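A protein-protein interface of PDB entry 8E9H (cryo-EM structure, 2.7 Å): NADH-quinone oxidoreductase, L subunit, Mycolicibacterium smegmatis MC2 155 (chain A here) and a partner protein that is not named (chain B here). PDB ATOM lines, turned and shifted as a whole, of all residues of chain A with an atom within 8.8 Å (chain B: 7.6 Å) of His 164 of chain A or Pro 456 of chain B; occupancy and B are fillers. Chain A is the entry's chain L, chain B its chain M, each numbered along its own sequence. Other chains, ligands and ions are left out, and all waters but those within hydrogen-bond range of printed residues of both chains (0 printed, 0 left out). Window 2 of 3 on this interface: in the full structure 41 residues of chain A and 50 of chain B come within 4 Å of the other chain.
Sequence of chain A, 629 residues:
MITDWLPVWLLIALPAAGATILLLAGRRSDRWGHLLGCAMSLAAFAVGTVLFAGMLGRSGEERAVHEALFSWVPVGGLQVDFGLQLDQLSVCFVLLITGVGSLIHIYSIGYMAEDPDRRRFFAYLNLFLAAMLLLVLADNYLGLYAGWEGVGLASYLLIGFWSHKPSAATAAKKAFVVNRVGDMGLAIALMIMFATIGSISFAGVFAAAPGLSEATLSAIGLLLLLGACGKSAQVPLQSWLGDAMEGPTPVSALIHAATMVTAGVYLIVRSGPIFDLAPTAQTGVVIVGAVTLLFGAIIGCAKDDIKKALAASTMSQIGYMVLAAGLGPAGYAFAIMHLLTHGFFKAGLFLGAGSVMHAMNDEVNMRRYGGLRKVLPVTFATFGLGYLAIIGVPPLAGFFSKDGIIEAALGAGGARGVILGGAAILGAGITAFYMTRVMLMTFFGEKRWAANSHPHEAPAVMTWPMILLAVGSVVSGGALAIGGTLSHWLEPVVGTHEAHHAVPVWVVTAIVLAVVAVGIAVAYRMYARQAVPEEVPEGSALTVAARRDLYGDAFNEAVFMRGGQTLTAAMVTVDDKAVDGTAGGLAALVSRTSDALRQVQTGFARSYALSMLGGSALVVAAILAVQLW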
ATOM      1  N   ASP A 115     -12.085  -5.716  -7.448  1.00  0.00           N
ATOM      2  CA  ASP A 115     -11.935  -4.270  -7.468  1.00  0.00           C
ATOM      3  C   ASP A 115     -12.436  -3.676  -6.164  1.00  0.00           C
ATOM      4  O   ASP A 115     -13.528  -4.042  -5.708  1.00  0.00           O
ATOM      5  CB  ASP A 115     -12.709  -3.664  -8.644  1.00  0.00           C
ATOM      6  N   PRO A 116     -11.691  -2.770  -5.531  1.00  0.00           N
ATOM      7  CA  PRO A 116     -12.193  -2.141  -4.308  1.00  0.00           C
ATOM      8  C   PRO A 116     -13.367  -1.224  -4.607  1.00  0.00           C
ATOM      9  O   PRO A 116     -13.687  -0.931  -5.760  1.00  0.00           O
ATOM     10  CB  PRO A 116     -10.984  -1.354  -3.789  1.00  0.00           C
ATOM     11  CG  PRO A 116     -10.184  -1.073  -5.005  1.00  0.00           C
ATOM     12  CD  PRO A 116     -10.348  -2.278  -5.882  1.00  0.00           C
ATOM     13  N   ARG A 120     -19.565   0.639  -2.959  1.00  0.00           N
ATOM     14  CA  ARG A 120     -20.014   1.910  -3.513  1.00  0.00           C
ATOM     15  C   ARG A 120     -20.583   1.730  -4.915  1.00  0.00           C
ATOM     16  O   ARG A 120     -21.574   2.374  -5.281  1.00  0.00           O
ATOM     17  CB  ARG A 120     -18.856   2.905  -3.525  1.00  0.00           C
ATOM     18  CG  ARG A 120     -19.252   4.303  -3.939  1.00  0.00           C
ATOM     19  CD  ARG A 120     -18.189   5.301  -3.544  1.00  0.00           C
ATOM     20  NE  ARG A 120     -16.908   4.991  -4.164  1.00  0.00           N
ATOM     21  CZ  ARG A 120     -16.558   5.361  -5.388  1.00  0.00           C
ATOM     22  NH1 ARG A 120     -17.380   6.046  -6.166  1.00  0.00           N
ATOM     23  NH2 ARG A 120     -15.354   5.032  -5.845  1.00  0.00           N
ATOM     24  N   ILE A 159     -20.772   5.693 -14.766  1.00  0.00           N
ATOM     25  CA  ILE A 159     -19.774   5.959 -15.796  1.00  0.00           C
ATOM     26  C   ILE A 159     -18.544   6.596 -15.172  1.00  0.00           C
ATOM     27  O   ILE A 159     -17.406   6.287 -15.544  1.00  0.00           O
ATOM     28  CB  ILE A 159     -20.369   6.854 -16.896  1.00  0.00           C
ATOM     29  CG1 ILE A 159     -21.508   6.132 -17.614  1.00  0.00           C
ATOM     30  CG2 ILE A 159     -19.290   7.255 -17.885  1.00  0.00           C
ATOM     31  CD1 ILE A 159     -22.410   7.056 -18.394  1.00  0.00           C
ATOM     32  N   GLY A 160     -18.752   7.489 -14.211  1.00  0.00           N
ATOM     33  CA  GLY A 160     -17.666   8.153 -13.531  1.00  0.00           C
ATOM     34  C   GLY A 160     -16.878   7.280 -12.590  1.00  0.00           C
ATOM     35  O   GLY A 160     -15.850   7.720 -12.071  1.00  0.00           O
ATOM     36  N   PHE A 161     -17.328   6.052 -12.349  1.00  0.00           N
ATOM     37  CA  PHE A 161     -16.560   5.138 -11.522  1.00  0.00           C
ATOM     38  C   PHE A 161     -15.153   4.991 -12.088  1.00  0.00           C
ATOM     39  O   PHE A 161     -14.888   5.306 -13.251  1.00  0.00           O
ATOM     40  CB  PHE A 161     -17.249   3.780 -11.442  1.00  0.00           C
ATOM     41  CG  PHE A 161     -16.936   3.022 -10.192  1.00  0.00           C
ATOM     42  CD1 PHE A 161     -17.605   3.302  -9.015  1.00  0.00           C
ATOM     43  CD2 PHE A 161     -15.972   2.034 -10.189  1.00  0.00           C
ATOM     44  CE1 PHE A 161     -17.319   2.607  -7.862  1.00  0.00           C
ATOM     45  CE2 PHE A 161     -15.682   1.336  -9.038  1.00  0.00           C
ATOM     46  CZ  PHE A 161     -16.356   1.623  -7.873  1.00  0.00           C
ATOM     47  N   TRP A 162     -14.240   4.508 -11.253  1.00  0.00           N
ATOM     48  CA  TRP A 162     -12.822   4.520 -11.590  1.00  0.00           C
ATOM     49  C   TRP A 162     -12.393   5.938 -11.949  1.00  0.00           C
ATOM     50  O   TRP A 162     -11.760   6.189 -12.976  1.00  0.00           O
ATOM     51  CB  TRP A 162     -12.516   3.551 -12.732  1.00  0.00           C
ATOM     52  CG  TRP A 162     -12.850   2.130 -12.430  1.00  0.00           C
ATOM     53  CD1 TRP A 162     -12.856   1.532 -11.206  1.00  0.00           C
ATOM     54  CD2 TRP A 162     -13.228   1.121 -13.371  1.00  0.00           C
ATOM     55  NE1 TRP A 162     -13.213   0.213 -11.326  1.00  0.00           N
ATOM     56  CE2 TRP A 162     -13.448  -0.064 -12.646  1.00  0.00           C
ATOM     57  CE3 TRP A 162     -13.402   1.106 -14.757  1.00  0.00           C
ATOM     58  CZ2 TRP A 162     -13.833  -1.253 -13.259  1.00  0.00           C
ATOM     59  CZ3 TRP A 162     -13.784  -0.075 -15.364  1.00  0.00           C
ATOM     60  CH2 TRP A 162     -13.995  -1.238 -14.616  1.00  0.00           C
ATOM     61  N   SER A 163     -12.755   6.881 -11.078  1.00  0.00           N
ATOM     62  CA  SER A 163     -12.526   8.291 -11.356  1.00  0.00           C
ATOM     63  C   SER A 163     -11.057   8.610 -11.579  1.00  0.00           C
ATOM     64  O   SER A 163     -10.753   9.635 -12.200  1.00  0.00           O
ATOM     65  CB  SER A 163     -13.065   9.142 -10.206  1.00  0.00           C
ATOM     66  N   HIS A 164     -10.143   7.773 -11.093  1.00  0.00           N
ATOM     67  CA  HIS A 164      -8.728   8.007 -11.344  1.00  0.00           C
ATOM     68  C   HIS A 164      -8.411   8.036 -12.832  1.00  0.00           C
ATOM     69  O   HIS A 164      -7.424   8.665 -13.229  1.00  0.00           O
ATOM     70  CB  HIS A 164      -7.885   6.937 -10.655  1.00  0.00           C
ATOM     71  CG  HIS A 164      -8.249   5.539 -11.044  1.00  0.00           C
ATOM     72  ND1 HIS A 164      -9.340   4.881 -10.520  1.00  0.00           N
ATOM     73  CD2 HIS A 164      -7.666   4.675 -11.907  1.00  0.00           C
ATOM     74  CE1 HIS A 164      -9.414   3.671 -11.045  1.00  0.00           C
ATOM     75  NE2 HIS A 164      -8.410   3.520 -11.888  1.00  0.00           N
ATOM     76  N   LYS A 165      -9.212   7.380 -13.656  1.00  0.00           N
ATOM     77  CA  LYS A 165      -9.014   7.423 -15.098  1.00  0.00           C
ATOM     78  C   LYS A 165      -9.677   8.671 -15.664  1.00  0.00           C
ATOM     79  O   LYS A 165     -10.909   8.775 -15.609  1.00  0.00           O
ATOM     80  CB  LYS A 165      -9.594   6.171 -15.748  1.00  0.00           C
ATOM     81  N   PRO A 166      -8.927   9.629 -16.216  1.00  0.00           N
ATOM     82  CA  PRO A 166      -9.572  10.856 -16.709  1.00  0.00           C
ATOM     83  C   PRO A 166     -10.618  10.602 -17.777  1.00  0.00           C
ATOM     84  O   PRO A 166     -11.606  11.343 -17.857  1.00  0.00           O
ATOM     85  CB  PRO A 166      -8.395  11.673 -17.257  1.00  0.00           C
ATOM     86  CG  PRO A 166      -7.202  11.145 -16.549  1.00  0.00           C
ATOM     87  CD  PRO A 166      -7.465   9.686 -16.360  1.00  0.00           C
ATOM     88  N   SER A 167     -10.424   9.578 -18.608  1.00  0.00           N
ATOM     89  CA  SER A 167     -11.391   9.293 -19.661  1.00  0.00           C
ATOM     90  C   SER A 167     -12.759   8.975 -19.075  1.00  0.00           C
ATOM     91  O   SER A 167     -13.786   9.409 -19.606  1.00  0.00           O
ATOM     92  CB  SER A 167     -10.894   8.137 -20.525  1.00  0.00           C
ATOM     93  OG  SER A 167     -10.651   6.986 -19.736  1.00  0.00           O
ATOM     94  N   ALA A 168     -12.794   8.213 -17.980  1.00  0.00           N
ATOM     95  CA  ALA A 168     -14.069   7.897 -17.351  1.00  0.00           C
ATOM     96  C   ALA A 168     -14.767   9.156 -16.855  1.00  0.00           C
ATOM     97  O   ALA A 168     -15.976   9.323 -17.055  1.00  0.00           O
ATOM     98  CB  ALA A 168     -13.856   6.916 -16.199  1.00  0.00           C
ATOM     99  N   ALA A 169     -14.026  10.053 -16.203  1.00  0.00           N
ATOM    100  CA  ALA A 169     -14.634  11.281 -15.706  1.00  0.00           C
ATOM    101  C   ALA A 169     -15.163  12.130 -16.853  1.00  0.00           C
ATOM    102  O   ALA A 169     -16.273  12.672 -16.777  1.00  0.00           O
ATOM    103  CB  ALA A 169     -13.620  12.071 -14.881  1.00  0.00           C
ATOM    104  N   GLU A 246     -16.174   3.846 -21.229  1.00  0.00           N
ATOM    105  CA  GLU A 246     -15.002   3.900 -20.366  1.00  0.00           C
ATOM    106  C   GLU A 246     -15.287   3.336 -18.982  1.00  0.00           C
ATOM    107  O   GLU A 246     -14.348   2.955 -18.275  1.00  0.00           O
ATOM    108  CB  GLU A 246     -14.507   5.343 -20.249  1.00  0.00           C
ATOM    109  N   TYR B 383      -6.043  21.317  -8.116  1.00  0.00           N
ATOM    110  CA  TYR B 383      -6.472  20.058  -7.529  1.00  0.00           C
ATOM    111  C   TYR B 383      -6.582  18.972  -8.593  1.00  0.00           C
ATOM    112  O   TYR B 383      -6.459  19.221  -9.793  1.00  0.00           O
ATOM    113  CB  TYR B 383      -7.813  20.231  -6.815  1.00  0.00           C
ATOM    114  CG  TYR B 383      -7.804  21.321  -5.775  1.00  0.00           C
ATOM    115  CD1 TYR B 383      -7.928  22.652  -6.139  1.00  0.00           C
ATOM    116  CD2 TYR B 383      -7.677  21.020  -4.431  1.00  0.00           C
ATOM    117  CE1 TYR B 383      -7.918  23.649  -5.195  1.00  0.00           C
ATOM    118  CE2 TYR B 383      -7.669  22.012  -3.479  1.00  0.00           C
ATOM    119  CZ  TYR B 383      -7.789  23.325  -3.867  1.00  0.00           C
ATOM    120  OH  TYR B 383      -7.781  24.321  -2.920  1.00  0.00           O
ATOM    121  N   GLY B 384      -6.821  17.750  -8.127  1.00  0.00           N
ATOM    122  CA  GLY B 384      -7.001  16.616  -9.011  1.00  0.00           C
ATOM    123  C   GLY B 384      -7.063  15.305  -8.258  1.00  0.00           C
ATOM    124  O   GLY B 384      -6.264  15.066  -7.348  1.00  0.00           O
ATOM    125  N   GLY B 385      -8.009  14.445  -8.625  1.00  0.00           N
ATOM    126  CA  GLY B 385      -8.118  13.149  -7.987  1.00  0.00           C
ATOM    127  C   GLY B 385      -8.360  13.202  -6.499  1.00  0.00           C
ATOM    128  O   GLY B 385      -7.953  12.285  -5.782  1.00  0.00           O
ATOM    129  N   VAL B 386      -9.023  14.249  -6.007  1.00  0.00           N
ATOM    130  CA  VAL B 386      -9.244  14.384  -4.576  1.00  0.00           C
ATOM    131  C   VAL B 386     -10.164  13.295  -4.042  1.00  0.00           C
ATOM    132  O   VAL B 386     -10.198  13.054  -2.833  1.00  0.00           O
ATOM    133  CB  VAL B 386      -9.805  15.786  -4.266  1.00  0.00           C
ATOM    134  CG1 VAL B 386     -10.223  15.887  -2.812  1.00  0.00           C
ATOM    135  CG2 VAL B 386      -8.779  16.853  -4.606  1.00  0.00           C
ATOM    136  N   GLN B 387     -10.914  12.624  -4.917  1.00  0.00           N
ATOM    137  CA  GLN B 387     -11.767  11.531  -4.461  1.00  0.00           C
ATOM    138  C   GLN B 387     -10.950  10.435  -3.797  1.00  0.00           C
ATOM    139  O   GLN B 387     -11.355   9.884  -2.767  1.00  0.00           O
ATOM    140  CB  GLN B 387     -12.560  10.951  -5.631  1.00  0.00           C
ATOM    141  CG  GLN B 387     -13.962  11.498  -5.767  1.00  0.00           C
ATOM    142  CD  GLN B 387     -14.840  10.618  -6.627  1.00  0.00           C
ATOM    143  OE1 GLN B 387     -14.383   9.621  -7.185  1.00  0.00           O
ATOM    144  NE2 GLN B 387     -16.111  10.981  -6.740  1.00  0.00           N
ATOM    145  N   LYS B 388      -9.799  10.100  -4.376  1.00  0.00           N
ATOM    146  CA  LYS B 388      -8.992   9.013  -3.835  1.00  0.00           C
ATOM    147  C   LYS B 388      -8.558   9.311  -2.406  1.00  0.00           C
ATOM    148  O   LYS B 388      -8.586   8.429  -1.542  1.00  0.00           O
ATOM    149  CB  LYS B 388      -7.775   8.772  -4.728  1.00  0.00           C
ATOM    150  N   ARG B 451     -12.473  18.466 -12.766  1.00  0.00           N
ATOM    151  CA  ARG B 451     -11.158  19.086 -12.677  1.00  0.00           C
ATOM    152  C   ARG B 451     -10.525  18.860 -11.311  1.00  0.00           C
ATOM    153  O   ARG B 451      -9.318  18.614 -11.215  1.00  0.00           O
ATOM    154  CB  ARG B 451     -11.265  20.578 -12.980  1.00  0.00           C
ATOM    155  CG  ARG B 451     -11.423  20.881 -14.456  1.00  0.00           C
ATOM    156  CD  ARG B 451     -11.521  22.369 -14.713  1.00  0.00           C
ATOM    157  NE  ARG B 451     -12.820  22.909 -14.332  1.00  0.00           N
ATOM    158  CZ  ARG B 451     -13.137  24.195 -14.380  1.00  0.00           C
ATOM    159  NH1 ARG B 451     -12.269  25.107 -14.786  1.00  0.00           N
ATOM    160  NH2 ARG B 451     -14.356  24.577 -14.012  1.00  0.00           N
ATOM    161  N   MET B 452     -11.316  18.938 -10.240  1.00  0.00           N
ATOM    162  CA  MET B 452     -10.754  18.879  -8.897  1.00  0.00           C
ATOM    163  C   MET B 452     -10.769  17.498  -8.261  1.00  0.00           C
ATOM    164  O   MET B 452      -9.804  17.150  -7.575  1.00  0.00           O
ATOM    165  CB  MET B 452     -11.495  19.841  -7.962  1.00  0.00           C
ATOM    166  CG  MET B 452     -11.601  21.254  -8.486  1.00  0.00           C
ATOM    167  SD  MET B 452     -12.064  22.442  -7.214  1.00  0.00           S
ATOM    168  CE  MET B 452     -13.061  21.447  -6.110  1.00  0.00           C
ATOM    169  N   MET B 453     -11.820  16.708  -8.462  1.00  0.00           N
ATOM    170  CA  MET B 453     -12.013  15.476  -7.720  1.00  0.00           C
ATOM    171  C   MET B 453     -11.526  14.237  -8.457  1.00  0.00           C
ATOM    172  O   MET B 453     -11.270  13.218  -7.808  1.00  0.00           O
ATOM    173  CB  MET B 453     -13.503  15.286  -7.400  1.00  0.00           C
ATOM    174  CG  MET B 453     -14.108  16.300  -6.443  1.00  0.00           C
ATOM    175  SD  MET B 453     -12.996  17.011  -5.225  1.00  0.00           S
ATOM    176  CE  MET B 453     -14.073  18.237  -4.496  1.00  0.00           C
ATOM    177  N   THR B 454     -11.389  14.291  -9.777  1.00  0.00           N
ATOM    178  CA  THR B 454     -11.120  13.111 -10.582  1.00  0.00           C
ATOM    179  C   THR B 454      -9.720  13.192 -11.172  1.00  0.00           C
ATOM    180  O   THR B 454      -9.008  14.187 -11.017  1.00  0.00           O
ATOM    181  CB  THR B 454     -12.147  12.956 -11.709  1.00  0.00           C
ATOM    182  OG1 THR B 454     -11.865  13.905 -12.745  1.00  0.00           O
ATOM    183  CG2 THR B 454     -13.553  13.180 -11.186  1.00  0.00           C
ATOM    184  N   GLY B 455      -9.334  12.121 -11.858  1.00  0.00           N
ATOM    185  CA  GLY B 455      -8.036  12.036 -12.478  1.00  0.00           C
ATOM    186  C   GLY B 455      -6.960  11.630 -11.493  1.00  0.00           C
ATOM    187  O   GLY B 455      -7.231  11.333 -10.327  1.00  0.00           O
ATOM    188  N   PRO B 456      -5.711  11.608 -11.950  1.00  0.00           N
ATOM    189  CA  PRO B 456      -4.612  11.236 -11.056  1.00  0.00           C
ATOM    190  C   PRO B 456      -4.475  12.228  -9.914  1.00  0.00           C
ATOM    191  O   PRO B 456      -4.694  13.430 -10.074  1.00  0.00           O
ATOM    192  CB  PRO B 456      -3.386  11.263 -11.972  1.00  0.00           C
ATOM    193  CG  PRO B 456      -3.753  12.223 -13.048  1.00  0.00           C
ATOM    194  CD  PRO B 456      -5.223  12.034 -13.271  1.00  0.00           C
ATOM    195  N   VAL B 457      -4.097  11.710  -8.748  1.00  0.00           N
ATOM    196  CA  VAL B 457      -3.910  12.551  -7.570  1.00  0.00           C
ATOM    197  C   VAL B 457      -2.758  13.507  -7.856  1.00  0.00           C
ATOM    198  O   VAL B 457      -1.610  13.082  -8.010  1.00  0.00           O
ATOM    199  CB  VAL B 457      -3.642  11.713  -6.317  1.00  0.00           C
ATOM    200  CG1 VAL B 457      -3.449  12.614  -5.113  1.00  0.00           C
ATOM    201  CG2 VAL B 457      -4.782  10.739  -6.079  1.00  0.00           C
ATOM    202  N   ARG B 458      -3.058  14.801  -7.924  1.00  0.00           N
ATOM    203  CA  ARG B 458      -2.039  15.786  -8.236  1.00  0.00           C
ATOM    204  C   ARG B 458      -1.006  15.861  -7.115  1.00  0.00           C
ATOM    205  O   ARG B 458      -1.267  15.501  -5.964  1.00  0.00           O
ATOM    206  CB  ARG B 458      -2.669  17.160  -8.462  1.00  0.00           C
ATOM    207  N   ASP B 459       0.184  16.337  -7.471  1.00  0.00           N
ATOM    208  CA  ASP B 459       1.279  16.408  -6.514  1.00  0.00           C
ATOM    209  C   ASP B 459       0.882  17.244  -5.304  1.00  0.00           C
ATOM    210  O   ASP B 459       0.295  18.321  -5.435  1.00  0.00           O
ATOM    211  CB  ASP B 459       2.520  17.002  -7.178  1.00  0.00           C
ATOM    212  N   ILE B 461      -1.351  16.553  -3.112  1.00  0.00           N
ATOM    213  CA  ILE B 461      -2.723  16.325  -2.674  1.00  0.00           C
ATOM    214  C   ILE B 461      -2.793  15.197  -1.657  1.00  0.00           C
ATOM    215  O   ILE B 461      -3.294  15.379  -0.544  1.00  0.00           O
ATOM    216  CB  ILE B 461      -3.622  16.035  -3.894  1.00  0.00           C
ATOM    217  CG1 ILE B 461      -3.668  17.244  -4.832  1.00  0.00           C
ATOM    218  CG2 ILE B 461      -5.022  15.659  -3.444  1.00  0.00           C
ATOM    219  CD1 ILE B 461      -4.477  18.406  -4.304  1.00  0.00           C
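Of the 15 printed residues of chain A, 4 touch a printed residue of chain B. Hydrophobic or aromatic side chains of chain A within 4 Å of the printed part of chain B: Pro 166 and Ala 169. Hydrophobic or aromatic side chains of chain B within 4 Å of the printed part of chain A: Pro 456. Along chain B the printed residues that touch a printed residue of chain A span positions 387 to 456.
The backbone NH (N) of Gln 387 of chain B is in hydrogen-bond range of the backbone carbonyl oxygen (O) of Met 453 of chain B, 3.0 Å away. The backbone NH (N) of Gly 385 of chain B sits at hydrogen-bond distance from the backbone carbonyl oxygen (O) of Thr 454 of chain B.
Among the printed residues, merely in contact across the chains: Ser 163 of chain A with Gln 387 of chain B, Ser 163 of chain A with Thr 454 of chain B, His 164 of chain A with Gly 455 of chain B, His 164 of chain A with Pro 456 of chain B, Pro 166 of chain A with Pro 456 of chain B and Ala 169 of chain A with Thr 454 of chain B.
Of the printed residues of chain B, Ser 163 of chain A touches Gln 387, Thr 454 and Gly 455. Of chain B, only Gly 455 (3.5 Å) and Pro 456 (3.6 Å) come within 4 Å of His 164 of chain A. Printed residues of chain B within 4 Å of Pro 166 of chain A: Pro 456. Of the printed residues of chain B, Ala 169 of chain A touches Thr 454 (3.3 Å). Of the printed residues of chain A, Gln 387 of chain B touches Ser 163. Printed residues of chain A within 4 Å of Thr 454 of chain B: Ser 163 and Ala 169. Pro 456 of chain B touches two residues of chain A. The nearest residue of chain B that does not touch His 164 of chain A is Thr 454 of chain B (5.3 Å).
The backbone NH (N) of Gly 455 of chain B sits at hydrogen-bond distance from the backbone carbonyl oxygen (O) of Ser 163 of chain A, 2.9 Å away.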
